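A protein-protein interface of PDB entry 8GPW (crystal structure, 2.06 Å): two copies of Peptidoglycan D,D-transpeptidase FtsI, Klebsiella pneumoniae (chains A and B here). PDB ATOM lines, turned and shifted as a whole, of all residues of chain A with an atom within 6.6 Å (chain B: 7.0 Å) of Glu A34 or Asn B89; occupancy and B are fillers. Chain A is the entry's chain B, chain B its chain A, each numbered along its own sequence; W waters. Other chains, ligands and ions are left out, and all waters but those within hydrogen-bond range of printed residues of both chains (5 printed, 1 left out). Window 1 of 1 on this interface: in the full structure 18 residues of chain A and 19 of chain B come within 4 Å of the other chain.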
ATOM      1  N   TYR A  29      -6.940 -22.596 -17.818  1.00  0.00           N
ATOM      2  CA  TYR A  29      -6.576 -23.566 -16.798  1.00  0.00           C
ATOM      3  C   TYR A  29      -6.196 -24.876 -17.471  1.00  0.00           C
ATOM      4  O   TYR A  29      -6.842 -25.294 -18.430  1.00  0.00           O
ATOM      5  CB  TYR A  29      -7.738 -23.781 -15.816  1.00  0.00           C
ATOM      6  CG  TYR A  29      -7.464 -24.787 -14.733  1.00  0.00           C
ATOM      7  CD1 TYR A  29      -6.610 -24.493 -13.677  1.00  0.00           C
ATOM      8  CD2 TYR A  29      -8.095 -26.029 -14.747  1.00  0.00           C
ATOM      9  CE1 TYR A  29      -6.382 -25.423 -12.676  1.00  0.00           C
ATOM     10  CE2 TYR A  29      -7.863 -26.958 -13.757  1.00  0.00           C
ATOM     11  CZ  TYR A  29      -7.000 -26.646 -12.721  1.00  0.00           C
ATOM     12  OH  TYR A  29      -6.770 -27.579 -11.730  1.00  0.00           O
ATOM     13  N   TYR A  30      -5.149 -25.525 -16.978  1.00  0.00           N
ATOM     14  CA  TYR A  30      -4.684 -26.779 -17.574  1.00  0.00           C
ATOM     15  C   TYR A  30      -4.865 -27.915 -16.577  1.00  0.00           C
ATOM     16  O   TYR A  30      -4.045 -28.064 -15.656  1.00  0.00           O
ATOM     17  CB  TYR A  30      -3.226 -26.632 -17.995  1.00  0.00           C
ATOM     18  CG  TYR A  30      -3.079 -25.516 -18.986  1.00  0.00           C
ATOM     19  CD1 TYR A  30      -3.360 -25.723 -20.340  1.00  0.00           C
ATOM     20  CD2 TYR A  30      -2.694 -24.236 -18.572  1.00  0.00           C
ATOM     21  CE1 TYR A  30      -3.250 -24.695 -21.248  1.00  0.00           C
ATOM     22  CE2 TYR A  30      -2.579 -23.211 -19.472  1.00  0.00           C
ATOM     23  CZ  TYR A  30      -2.857 -23.440 -20.807  1.00  0.00           C
ATOM     24  OH  TYR A  30      -2.763 -22.417 -21.706  1.00  0.00           O
ATOM     25  N   SER A  32      -4.386 -31.115 -16.421  1.00  0.00           N
ATOM     26  CA  SER A  32      -3.359 -32.104 -16.136  1.00  0.00           C
ATOM     27  C   SER A  32      -2.030 -31.435 -15.804  1.00  0.00           C
ATOM     28  O   SER A  32      -1.038 -32.134 -15.565  1.00  0.00           O
ATOM     29  CB  SER A  32      -3.173 -33.076 -17.298  1.00  0.00           C
ATOM     30  OG  SER A  32      -2.427 -32.452 -18.326  1.00  0.00           O
ATOM     31  N   GLY A  33      -1.992 -30.101 -15.795  1.00  0.00           N
ATOM     32  CA  GLY A  33      -0.804 -29.369 -15.391  1.00  0.00           C
ATOM     33  C   GLY A  33       0.448 -29.868 -16.071  1.00  0.00           C
ATOM     34  O   GLY A  33       0.513 -29.888 -17.295  1.00  0.00           O
ATOM     35  N   GLU A  34       1.452 -30.301 -15.309  1.00  0.00           N
ATOM     36  CA  GLU A  34       2.745 -30.567 -15.934  1.00  0.00           C
ATOM     37  C   GLU A  34       2.783 -31.904 -16.688  1.00  0.00           C
ATOM     38  O   GLU A  34       3.705 -32.100 -17.494  1.00  0.00           O
ATOM     39  CB  GLU A  34       3.837 -30.380 -14.874  1.00  0.00           C
ATOM     40  CG  GLU A  34       3.902 -31.350 -13.757  1.00  0.00           C
ATOM     41  CD  GLU A  34       2.836 -31.085 -12.661  1.00  0.00           C
ATOM     42  OE1 GLU A  34       1.850 -30.412 -12.955  1.00  0.00           O
ATOM     43  OE2 GLU A  34       3.067 -31.502 -11.488  1.00  0.00           O
ATOM     44  N   VAL A  35       1.804 -32.782 -16.471  1.00  0.00           N
ATOM     45  CA  VAL A  35       1.700 -34.039 -17.202  1.00  0.00           C
ATOM     46  C   VAL A  35       1.702 -33.813 -18.716  1.00  0.00           C
ATOM     47  O   VAL A  35       2.324 -34.572 -19.463  1.00  0.00           O
ATOM     48  CB  VAL A  35       0.438 -34.790 -16.731  1.00  0.00           C
ATOM     49  CG1 VAL A  35       0.118 -36.020 -17.649  1.00  0.00           C
ATOM     50  CG2 VAL A  35       0.577 -35.232 -15.262  1.00  0.00           C
ATOM     51  N   THR A  36       1.007 -32.791 -19.197  1.00  0.00           N
ATOM     52  CA  THR A  36       0.880 -32.610 -20.642  1.00  0.00           C
ATOM     53  C   THR A  36       1.373 -31.233 -21.073  1.00  0.00           C
ATOM     54  O   THR A  36       0.947 -30.720 -22.112  1.00  0.00           O
ATOM     55  CB  THR A  36      -0.574 -32.831 -21.083  1.00  0.00           C
ATOM     56  OG1 THR A  36      -1.129 -33.921 -20.352  1.00  0.00           O
ATOM     57  CG2 THR A  36      -0.642 -33.201 -22.579  1.00  0.00           C
ATOM     58  N   ALA A  37       2.306 -30.637 -20.300  1.00  0.00           N
ATOM     59  CA  ALA A  37       2.651 -29.224 -20.469  1.00  0.00           C
ATOM     60  C   ALA A  37       3.341 -28.940 -21.803  1.00  0.00           C
ATOM     61  O   ALA A  37       3.051 -27.928 -22.455  1.00  0.00           O
ATOM     62  CB  ALA A  37       3.545 -28.757 -19.303  1.00  0.00           C
ATOM     63  N   HIS A  38       4.299 -29.774 -22.206  1.00  0.00           N
ATOM     64  CA  HIS A  38       5.058 -29.442 -23.406  1.00  0.00           C
ATOM     65  C   HIS A  38       4.181 -29.505 -24.648  1.00  0.00           C
ATOM     66  O   HIS A  38       4.311 -28.678 -25.554  1.00  0.00           O
ATOM     67  CB  HIS A  38       6.256 -30.378 -23.551  1.00  0.00           C
ATOM     68  CG  HIS A  38       7.270 -30.207 -22.470  1.00  0.00           C
ATOM     69  ND1 HIS A  38       7.445 -31.132 -21.466  1.00  0.00           N
ATOM     70  CD2 HIS A  38       8.144 -29.201 -22.220  1.00  0.00           C
ATOM     71  CE1 HIS A  38       8.394 -30.710 -20.647  1.00  0.00           C
ATOM     72  NE2 HIS A  38       8.835 -29.544 -21.083  1.00  0.00           N
ATOM     73  N   GLN A  81      -1.002 -40.759 -21.131  1.00  0.00           N
ATOM     74  CA  GLN A  81      -0.088 -39.638 -20.888  1.00  0.00           C
ATOM     75  C   GLN A  81       0.350 -39.599 -19.425  1.00  0.00           C
ATOM     76  O   GLN A  81       1.538 -39.421 -19.120  1.00  0.00           O
ATOM     77  CB  GLN A  81      -0.753 -38.315 -21.268  1.00  0.00           C
ATOM     78  CG  GLN A  81       0.113 -37.105 -21.028  1.00  0.00           C
ATOM     79  CD  GLN A  81       1.146 -36.889 -22.123  1.00  0.00           C
ATOM     80  OE1 GLN A  81       1.043 -37.477 -23.210  1.00  0.00           O
ATOM     81  NE2 GLN A  81       2.143 -36.019 -21.853  1.00  0.00           N
ATOM     82  N   TYR A  85       4.138 -40.164 -18.161  1.00  0.00           N
ATOM     83  CA  TYR A  85       4.859 -39.116 -17.446  1.00  0.00           C
ATOM     84  C   TYR A  85       5.347 -39.606 -16.088  1.00  0.00           C
ATOM     85  O   TYR A  85       6.494 -39.343 -15.695  1.00  0.00           O
ATOM     86  CB  TYR A  85       3.979 -37.886 -17.252  1.00  0.00           C
ATOM     87  CG  TYR A  85       4.707 -36.782 -16.485  1.00  0.00           C
ATOM     88  CD1 TYR A  85       5.690 -36.003 -17.117  1.00  0.00           C
ATOM     89  CD2 TYR A  85       4.437 -36.529 -15.140  1.00  0.00           C
ATOM     90  CE1 TYR A  85       6.355 -34.995 -16.437  1.00  0.00           C
ATOM     91  CE2 TYR A  85       5.119 -35.516 -14.446  1.00  0.00           C
ATOM     92  CZ  TYR A  85       6.072 -34.762 -15.098  1.00  0.00           C
ATOM     93  OH  TYR A  85       6.747 -33.752 -14.432  1.00  0.00           O
ATOM     94  N   ASN A 117       7.768 -35.341 -21.465  1.00  0.00           N
ATOM     95  CA  ASN A 117       9.158 -34.989 -21.211  1.00  0.00           C
ATOM     96  C   ASN A 117       9.353 -34.717 -19.725  1.00  0.00           C
ATOM     97  O   ASN A 117       8.415 -34.336 -19.018  1.00  0.00           O
ATOM     98  CB  ASN A 117       9.611 -33.750 -22.002  1.00  0.00           C
ATOM     99  CG  ASN A 117       9.412 -33.899 -23.520  1.00  0.00           C
ATOM    100  OD1 ASN A 117      10.172 -34.588 -24.199  1.00  0.00           O
ATOM    101  ND2 ASN A 117       8.405 -33.225 -24.045  1.00  0.00           N
ATOM    102  N   SER A 120       9.409 -31.202 -16.557  1.00  0.00           N
ATOM    103  CA  SER A 120       8.267 -30.443 -17.014  1.00  0.00           C
ATOM    104  C   SER A 120       8.078 -29.255 -16.070  1.00  0.00           C
ATOM    105  O   SER A 120       8.931 -28.957 -15.226  1.00  0.00           O
ATOM    106  CB  SER A 120       7.037 -31.351 -17.082  1.00  0.00           C
ATOM    107  OG  SER A 120       5.943 -30.691 -17.697  1.00  0.00           O
ATOM    108  N   TYR A 121       6.943 -28.582 -16.202  1.00  0.00           N
ATOM    109  CA  TYR A 121       6.643 -27.380 -15.435  1.00  0.00           C
ATOM    110  C   TYR A 121       5.131 -27.270 -15.378  1.00  0.00           C
ATOM    111  O   TYR A 121       4.420 -27.935 -16.132  1.00  0.00           O
ATOM    112  CB  TYR A 121       7.251 -26.129 -16.082  1.00  0.00           C
ATOM    113  CG  TYR A 121       6.632 -25.861 -17.450  1.00  0.00           C
ATOM    114  CD1 TYR A 121       6.990 -26.618 -18.559  1.00  0.00           C
ATOM    115  CD2 TYR A 121       5.669 -24.867 -17.624  1.00  0.00           C
ATOM    116  CE1 TYR A 121       6.423 -26.392 -19.795  1.00  0.00           C
ATOM    117  CE2 TYR A 121       5.092 -24.629 -18.862  1.00  0.00           C
ATOM    118  CZ  TYR A 121       5.465 -25.406 -19.948  1.00  0.00           C
ATOM    119  OH  TYR A 121       4.895 -25.192 -21.192  1.00  0.00           O
ATOM    120  N   ASN A 122       4.640 -26.402 -14.504  1.00  0.00           N
ATOM    121  CA  ASN A 122       3.202 -26.254 -14.411  1.00  0.00           C
ATOM    122  C   ASN A 122       2.734 -25.079 -15.269  1.00  0.00           C
ATOM    123  O   ASN A 122       3.010 -23.914 -14.927  1.00  0.00           O
ATOM    124  CB  ASN A 122       2.750 -26.092 -12.963  1.00  0.00           C
ATOM    125  CG  ASN A 122       1.270 -26.409 -12.810  1.00  0.00           C
ATOM    126  OD1 ASN A 122       0.462 -25.936 -13.612  1.00  0.00           O
ATOM    127  ND2 ASN A 122       0.910 -27.227 -11.821  1.00  0.00           N
ATOM    128  N   PRO A 123       2.031 -25.334 -16.382  1.00  0.00           N
ATOM    129  CA  PRO A 123       1.567 -24.237 -17.240  1.00  0.00           C
ATOM    130  C   PRO A 123       0.519 -23.363 -16.581  1.00  0.00           C
ATOM    131  O   PRO A 123       0.220 -22.279 -17.102  1.00  0.00           O
ATOM    132  CB  PRO A 123       0.980 -24.974 -18.456  1.00  0.00           C
ATOM    133  CG  PRO A 123       0.512 -26.284 -17.892  1.00  0.00           C
ATOM    134  CD  PRO A 123       1.542 -26.645 -16.856  1.00  0.00           C
ATOM    135  N   ASN A 124      -0.061 -23.800 -15.469  1.00  0.00           N
ATOM    136  CA  ASN A 124      -0.953 -22.944 -14.703  1.00  0.00           C
ATOM    137  C   ASN A 124      -0.217 -21.791 -14.030  1.00  0.00           C
ATOM    138  O   ASN A 124      -0.859 -20.842 -13.567  1.00  0.00           O
ATOM    139  CB  ASN A 124      -1.692 -23.796 -13.674  1.00  0.00           C
ATOM    140  CG  ASN A 124      -2.659 -24.786 -14.338  1.00  0.00           C
ATOM    141  OD1 ASN A 124      -3.535 -24.383 -15.103  1.00  0.00           O
ATOM    142  ND2 ASN A 124      -2.491 -26.072 -14.052  1.00  0.00           N
ATOM    143  N   GLU B  34       6.664 -36.962  -6.476  1.00  0.00           N
ATOM    144  CA  GLU B  34       6.268 -35.798  -5.692  1.00  0.00           C
ATOM    145  C   GLU B  34       4.826 -35.887  -5.182  1.00  0.00           C
ATOM    146  O   GLU B  34       4.442 -35.092  -4.322  1.00  0.00           O
ATOM    147  CB  GLU B  34       6.481 -34.540  -6.537  1.00  0.00           C
ATOM    148  CG  GLU B  34       5.396 -34.309  -7.569  1.00  0.00           C
ATOM    149  CD  GLU B  34       5.623 -35.064  -8.891  1.00  0.00           C
ATOM    150  OE1 GLU B  34       6.384 -36.074  -8.914  1.00  0.00           O
ATOM    151  OE2 GLU B  34       5.026 -34.640  -9.914  1.00  0.00           O
ATOM    152  N   VAL B  84      -6.186 -36.099  -5.434  1.00  0.00           N
ATOM    153  CA  VAL B  84      -6.116 -34.977  -4.492  1.00  0.00           C
ATOM    154  C   VAL B  84      -4.951 -34.064  -4.855  1.00  0.00           C
ATOM    155  O   VAL B  84      -5.114 -32.845  -5.002  1.00  0.00           O
ATOM    156  CB  VAL B  84      -6.004 -35.488  -3.034  1.00  0.00           C
ATOM    157  CG1 VAL B  84      -5.584 -34.340  -2.056  1.00  0.00           C
ATOM    158  CG2 VAL B  84      -7.298 -36.147  -2.562  1.00  0.00           C
ATOM    159  N   TYR B  85      -3.757 -34.641  -5.015  1.00  0.00           N
ATOM    160  CA  TYR B  85      -2.578 -33.844  -5.369  1.00  0.00           C
ATOM    161  C   TYR B  85      -2.757 -33.112  -6.705  1.00  0.00           C
ATOM    162  O   TYR B  85      -2.308 -31.968  -6.869  1.00  0.00           O
ATOM    163  CB  TYR B  85      -1.348 -34.744  -5.434  1.00  0.00           C
ATOM    164  CG  TYR B  85      -0.122 -33.970  -5.833  1.00  0.00           C
ATOM    165  CD1 TYR B  85       0.553 -33.187  -4.905  1.00  0.00           C
ATOM    166  CD2 TYR B  85       0.336 -33.981  -7.149  1.00  0.00           C
ATOM    167  CE1 TYR B  85       1.678 -32.447  -5.270  1.00  0.00           C
ATOM    168  CE2 TYR B  85       1.442 -33.248  -7.528  1.00  0.00           C
ATOM    169  CZ  TYR B  85       2.113 -32.482  -6.576  1.00  0.00           C
ATOM    170  OH  TYR B  85       3.212 -31.765  -6.932  1.00  0.00           O
ATOM    171  N   ARG B  86      -3.378 -33.779  -7.679  1.00  0.00           N
ATOM    172  CA  ARG B  86      -3.605 -33.185  -8.996  1.00  0.00           C
ATOM    173  C   ARG B  86      -4.396 -31.898  -8.878  1.00  0.00           C
ATOM    174  O   ARG B  86      -3.973 -30.840  -9.361  1.00  0.00           O
ATOM    175  CB  ARG B  86      -4.354 -34.182  -9.889  1.00  0.00           C
ATOM    176  CG  ARG B  86      -4.749 -33.665 -11.280  1.00  0.00           C
ATOM    177  CD  ARG B  86      -5.602 -34.750 -11.963  1.00  0.00           C
ATOM    178  NE  ARG B  86      -5.749 -34.594 -13.413  1.00  0.00           N
ATOM    179  CZ  ARG B  86      -6.749 -33.940 -13.984  1.00  0.00           C
ATOM    180  NH1 ARG B  86      -7.681 -33.376 -13.228  1.00  0.00           N
ATOM    181  NH2 ARG B  86      -6.823 -33.858 -15.301  1.00  0.00           N
ATOM    182  N   GLU B  87      -5.562 -31.971  -8.239  1.00  0.00           N
ATOM    183  CA  GLU B  87      -6.375 -30.771  -8.081  1.00  0.00           C
ATOM    184  C   GLU B  87      -5.661 -29.724  -7.231  1.00  0.00           C
ATOM    185  O   GLU B  87      -5.669 -28.535  -7.559  1.00  0.00           O
ATOM    186  CB  GLU B  87      -7.723 -31.138  -7.461  1.00  0.00           C
ATOM    187  CG  GLU B  87      -8.508 -32.187  -8.247  1.00  0.00           C
ATOM    188  CD  GLU B  87      -8.593 -31.822  -9.755  1.00  0.00           C
ATOM    189  OE1 GLU B  87      -8.925 -30.671 -10.080  1.00  0.00           O
ATOM    190  OE2 GLU B  87      -8.320 -32.687 -10.591  1.00  0.00           O
ATOM    191  N   LEU B  88      -5.064 -30.142  -6.112  1.00  0.00           N
ATOM    192  CA  LEU B  88      -4.507 -29.167  -5.175  1.00  0.00           C
ATOM    193  C   LEU B  88      -3.331 -28.430  -5.799  1.00  0.00           C
ATOM    194  O   LEU B  88      -3.276 -27.189  -5.799  1.00  0.00           O
ATOM    195  CB  LEU B  88      -4.078 -29.876  -3.879  1.00  0.00           C
ATOM    196  CG  LEU B  88      -3.368 -29.000  -2.864  1.00  0.00           C
ATOM    197  CD1 LEU B  88      -4.361 -27.981  -2.297  1.00  0.00           C
ATOM    198  CD2 LEU B  88      -2.718 -29.862  -1.752  1.00  0.00           C
ATOM    199  N   ASN B  89      -2.382 -29.195  -6.344  1.00  0.00           N
ATOM    200  CA  ASN B  89      -1.183 -28.638  -6.960  1.00  0.00           C
ATOM    201  C   ASN B  89      -1.521 -27.697  -8.118  1.00  0.00           C
ATOM    202  O   ASN B  89      -0.995 -26.582  -8.202  1.00  0.00           O
ATOM    203  CB  ASN B  89      -0.289 -29.795  -7.414  1.00  0.00           C
ATOM    204  CG  ASN B  89       1.001 -29.333  -8.044  1.00  0.00           C
ATOM    205  OD1 ASN B  89       1.812 -28.647  -7.414  1.00  0.00           O
ATOM    206  ND2 ASN B  89       1.197 -29.705  -9.307  1.00  0.00           N
ATOM    207  N   ASN B  90      -2.451 -28.091  -8.990  1.00  0.00           N
ATOM    208  CA  ASN B  90      -2.792 -27.160 -10.057  1.00  0.00           C
ATOM    209  C   ASN B  90      -3.555 -25.943  -9.541  1.00  0.00           C
ATOM    210  O   ASN B  90      -3.423 -24.848 -10.109  1.00  0.00           O
ATOM    211  CB  ASN B  90      -3.563 -27.905 -11.150  1.00  0.00           C
ATOM    212  CG  ASN B  90      -2.675 -28.904 -11.863  1.00  0.00           C
ATOM    213  OD1 ASN B  90      -1.604 -28.539 -12.351  1.00  0.00           O
ATOM    214  ND2 ASN B  90      -3.120 -30.156 -11.956  1.00  0.00           N
ATOM    215  N   ALA B  91      -4.336 -26.094  -8.461  1.00  0.00           N
ATOM    216  CA  ALA B  91      -5.004 -24.932  -7.871  1.00  0.00           C
ATOM    217  C   ALA B  91      -4.004 -23.970  -7.243  1.00  0.00           C
ATOM    218  O   ALA B  91      -4.183 -22.750  -7.315  1.00  0.00           O
ATOM    219  CB  ALA B  91      -6.020 -25.371  -6.818  1.00  0.00           C
ATOM    220  N   VAL B  92      -2.969 -24.495  -6.583  1.00  0.00           N
ATOM    221  CA  VAL B  92      -1.981 -23.608  -5.973  1.00  0.00           C
ATOM    222  C   VAL B  92      -1.271 -22.816  -7.065  1.00  0.00           C
ATOM    223  O   VAL B  92      -1.125 -21.591  -6.975  1.00  0.00           O
ATOM    224  CB  VAL B  92      -0.996 -24.409  -5.096  1.00  0.00           C
ATOM    225  CG1 VAL B  92       0.234 -23.519  -4.678  1.00  0.00           C
ATOM    226  CG2 VAL B  92      -1.713 -24.974  -3.850  1.00  0.00           C
ATOM    227  N   ALA B  93      -0.890 -23.500  -8.150  1.00  0.00           N
ATOM    228  CA  ALA B  93      -0.244 -22.837  -9.274  1.00  0.00           C
ATOM    229  C   ALA B  93      -1.166 -21.802  -9.900  1.00  0.00           C
ATOM    230  O   ALA B  93      -0.783 -20.641 -10.086  1.00  0.00           O
ATOM    231  CB  ALA B  93       0.176 -23.881 -10.310  1.00  0.00           C
ATOM    232  N   PHE B  94      -2.396 -22.211 -10.219  1.00  0.00           N
ATOM    233  CA  PHE B  94      -3.348 -21.324 -10.879  1.00  0.00           C
ATOM    234  C   PHE B  94      -3.613 -20.077 -10.051  1.00  0.00           C
ATOM    235  O   PHE B  94      -3.743 -18.973 -10.595  1.00  0.00           O
ATOM    236  CB  PHE B  94      -4.653 -22.075 -11.114  1.00  0.00           C
ATOM    237  CG  PHE B  94      -5.679 -21.285 -11.861  1.00  0.00           C
ATOM    238  CD1 PHE B  94      -5.555 -21.081 -13.231  1.00  0.00           C
ATOM    239  CD2 PHE B  94      -6.783 -20.762 -11.203  1.00  0.00           C
ATOM    240  CE1 PHE B  94      -6.514 -20.363 -13.927  1.00  0.00           C
ATOM    241  CE2 PHE B  94      -7.748 -20.037 -11.899  1.00  0.00           C
ATOM    242  CZ  PHE B  94      -7.615 -19.846 -13.259  1.00  0.00           C
ATOM    243  N   ASN B  95      -3.718 -20.240  -8.737  1.00  0.00           N
ATOM    244  CA  ASN B  95      -3.980 -19.129  -7.834  1.00  0.00           C
ATOM    245  C   ASN B  95      -2.718 -18.386  -7.405  1.00  0.00           C
ATOM    246  O   ASN B  95      -2.819 -17.468  -6.582  1.00  0.00           O
ATOM    247  CB  ASN B  95      -4.714 -19.655  -6.605  1.00  0.00           C
ATOM    248  CG  ASN B  95      -6.185 -19.860  -6.860  1.00  0.00           C
ATOM    249  OD1 ASN B  95      -6.943 -18.901  -6.952  1.00  0.00           O
ATOM    250  ND2 ASN B  95      -6.592 -21.114  -7.010  1.00  0.00           N
ATOM    251  N   GLY B 100      -0.471 -24.992  -0.568  1.00  0.00           N
ATOM    252  CA  GLY B 100      -1.759 -25.575  -0.242  1.00  0.00           C
ATOM    253  C   GLY B 100      -1.616 -26.950   0.386  1.00  0.00           C
ATOM    254  O   GLY B 100      -0.651 -27.680   0.124  1.00  0.00           O
ATOM    255  N   ALA B 116      -1.820 -34.385   1.045  1.00  0.00           N
ATOM    256  CA  ALA B 116      -1.023 -33.823  -0.038  1.00  0.00           C
ATOM    257  C   ALA B 116      -0.768 -32.355   0.233  1.00  0.00           C
ATOM    258  O   ALA B 116      -1.592 -31.673   0.845  1.00  0.00           O
ATOM    259  CB  ALA B 116      -1.718 -33.953  -1.397  1.00  0.00           C
ATOM    260  N   ASN B 117       0.365 -31.871  -0.268  1.00  0.00           N
ATOM    261  CA  ASN B 117       0.720 -30.465  -0.192  1.00  0.00           C
ATOM    262  C   ASN B 117       1.312 -30.039  -1.525  1.00  0.00           C
ATOM    263  O   ASN B 117       1.879 -30.850  -2.258  1.00  0.00           O
ATOM    264  CB  ASN B 117       1.755 -30.164   0.905  1.00  0.00           C
ATOM    265  CG  ASN B 117       1.390 -30.776   2.255  1.00  0.00           C
ATOM    266  OD1 ASN B 117       0.611 -30.215   3.010  1.00  0.00           O
ATOM    267  ND2 ASN B 117       1.987 -31.903   2.564  1.00  0.00           N
ATOM    268  N   SER B 118       1.205 -28.739  -1.806  1.00  0.00           N
ATOM    269  CA  SER B 118       1.858 -28.100  -2.936  1.00  0.00           C
ATOM    270  C   SER B 118       2.414 -26.787  -2.406  1.00  0.00           C
ATOM    271  O   SER B 118       1.736 -26.103  -1.632  1.00  0.00           O
ATOM    272  CB  SER B 118       0.885 -27.852  -4.100  1.00  0.00           C
ATOM    273  OG  SER B 118       1.508 -27.264  -5.241  1.00  0.00           O
ATOM    274  N   PRO B 119       3.642 -26.418  -2.776  1.00  0.00           N
ATOM    275  CA  PRO B 119       4.537 -27.131  -3.687  1.00  0.00           C
ATOM    276  C   PRO B 119       5.115 -28.414  -3.105  1.00  0.00           C
ATOM    277  O   PRO B 119       5.267 -28.574  -1.882  1.00  0.00           O
ATOM    278  CB  PRO B 119       5.669 -26.111  -3.920  1.00  0.00           C
ATOM    279  CG  PRO B 119       5.730 -25.382  -2.641  1.00  0.00           C
ATOM    280  CD  PRO B 119       4.287 -25.215  -2.230  1.00  0.00           C
ATOM    281  N   SER B 120       5.479 -29.321  -3.996  1.00  0.00           N
ATOM    282  CA  SER B 120       6.112 -30.563  -3.603  1.00  0.00           C
ATOM    283  C   SER B 120       7.494 -30.619  -4.237  1.00  0.00           C
ATOM    284  O   SER B 120       7.957 -29.650  -4.832  1.00  0.00           O
ATOM    285  CB  SER B 120       5.255 -31.761  -4.007  1.00  0.00           C
ATOM    286  OG  SER B 120       5.699 -32.927  -3.336  1.00  0.00           O
ATOM    287  N   VAL B 389     -12.060 -26.449  -5.730  1.00  0.00           N
ATOM    288  CA  VAL B 389     -11.096 -27.526  -5.526  1.00  0.00           C
ATOM    289  C   VAL B 389     -11.701 -28.628  -4.676  1.00  0.00           C
ATOM    290  O   VAL B 389     -11.515 -29.825  -4.950  1.00  0.00           O
ATOM    291  CB  VAL B 389      -9.810 -26.972  -4.886  1.00  0.00           C
ATOM    292  CG1 VAL B 389      -8.753 -28.069  -4.818  1.00  0.00           C
ATOM    293  CG2 VAL B 389      -9.291 -25.735  -5.664  1.00  0.00           C
HETATM  294  O   HOH W   1      -6.803 -30.217 -12.247  1.00  0.00           O
HETATM  295  O   HOH W   2       5.919 -33.382 -12.075  1.00  0.00           O
HETATM  296  O   HOH W   3      -0.342 -31.268 -10.792  1.00  0.00           O
HETATM  297  O   HOH W   4       4.253 -32.003  -9.318  1.00  0.00           O
HETATM  298  O   HOH W   5      -7.472 -27.071  -9.267  1.00  0.00           O
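Of the printed residues of chain B, Asn A122 touches Asn B89 (3.5 Å), Asn B90 (2.9 Å) and Ala B93 (3.7 Å). Printed residues of chain A within 4 Å of Arg B86: Ser A32. Asn B89 touches just these residues of chain A: Glu A34 (3.4 Å) and Asn A122 (3.5 Å). Of the printed residues of chain A, Asn B90 touches Tyr A29, Gly A33, Glu A34, Asn A122 and Asn A124. Of the printed residues of chain A, Phe B94 touches Tyr A29 and Asn A124. Asn B95 touches none of the printed residues of chain A. The nearest residue of chain B that does not touch Glu A34 is Glu B34 (4.02 Å).
Water W4 lies within hydrogen-bond range of OE2 of Glu A34 (2.5 Å), OH of Tyr B85 (2.6 Å) and OE2 of Glu B34 (2.8 Å). Water W2 lies within hydrogen-bond range of OH of Tyr A85 (2.5 Å), OE2 of Glu B34 (2.7 Å) and OE2 of Glu A34 (3.5 Å). Water W5 lies within hydrogen-bond range of the side-chain hydroxyl of Tyr A29, the backbone carbonyl oxygen of Glu B87 and the backbone NH of Ala B91. Water W3 lies within hydrogen-bond range of the side-chain amide nitrogen of Asn B89 (2.6 Å), the side-chain carboxylate of Glu A34 (3.2 Å) and the side-chain amide nitrogen of Asn B90 (3.2 Å). Water W1 lies within hydrogen-bond range of the side-chain hydroxyl of Tyr A29, the side-chain carboxylate of Glu B87 and the guanidinium group of Arg B86.
Printed residues of chain A that touch a printed residue of chain B: Tyr A29, Ser A32, Gly A33, Glu A34, Asn A122 and Asn A124. Among the printed residues, no Asp or Glu carboxylate lies within 4 Å of a Lys or Arg side-chain nitrogen of the other chain.
OD1 of Asn A122 is in hydrogen-bond range of N of Asn A124 (2.9 Å). The side-chain hydroxyl (OG) of Ser A32 sits at hydrogen-bond distance from the side-chain hydroxyl (OG1) of Thr A36, at 2.8 Å. ND2 of Asn B90 is in hydrogen-bond range of O of Arg B86 (2.8 Å). The backbone NH of Tyr A30 is in hydrogen-bond range of the side-chain amide oxygen of Asn A124. OE2 of Glu B87 is in salt-bridge range of NH1 of Arg B86. The side-chain amide oxygen (OD1) of Asn B89 is in hydrogen-bond range of the side-chain hydroxyl (OG) of Ser B118 (2.6 Å).
OE2 of Glu A34 is in hydrogen-bond range of ND2 of Asn B89 (3.4 Å). The side-chain amide oxygen of Asn B90 sits at hydrogen-bond distance from the side-chain amide nitrogen of Asn A122 (2.9 Å). ND2 of Asn A124 sits at hydrogen-bond distance from OD1 of Asn B90 (3.1 Å). O of Asn A124 lies close to O of Ala B93, at 3.5 Å.
Among the printed residues, merely in contact across the chains: Gly A33 with Asn B90, Tyr A29 with Asn B90, Asn A122 with Asn B89, Tyr A29 with Phe B94, Asn A124 with Phe B94, Asn A122 with Ala B93, Ser A32 with Arg B86 and Glu A34 with Asn B90.
Positions printed for both chains: 34, 85, 117 and 120. Of the 12 pairs that touch across the chains among the printed residues, none has its exchanged pair printed and touching as well.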
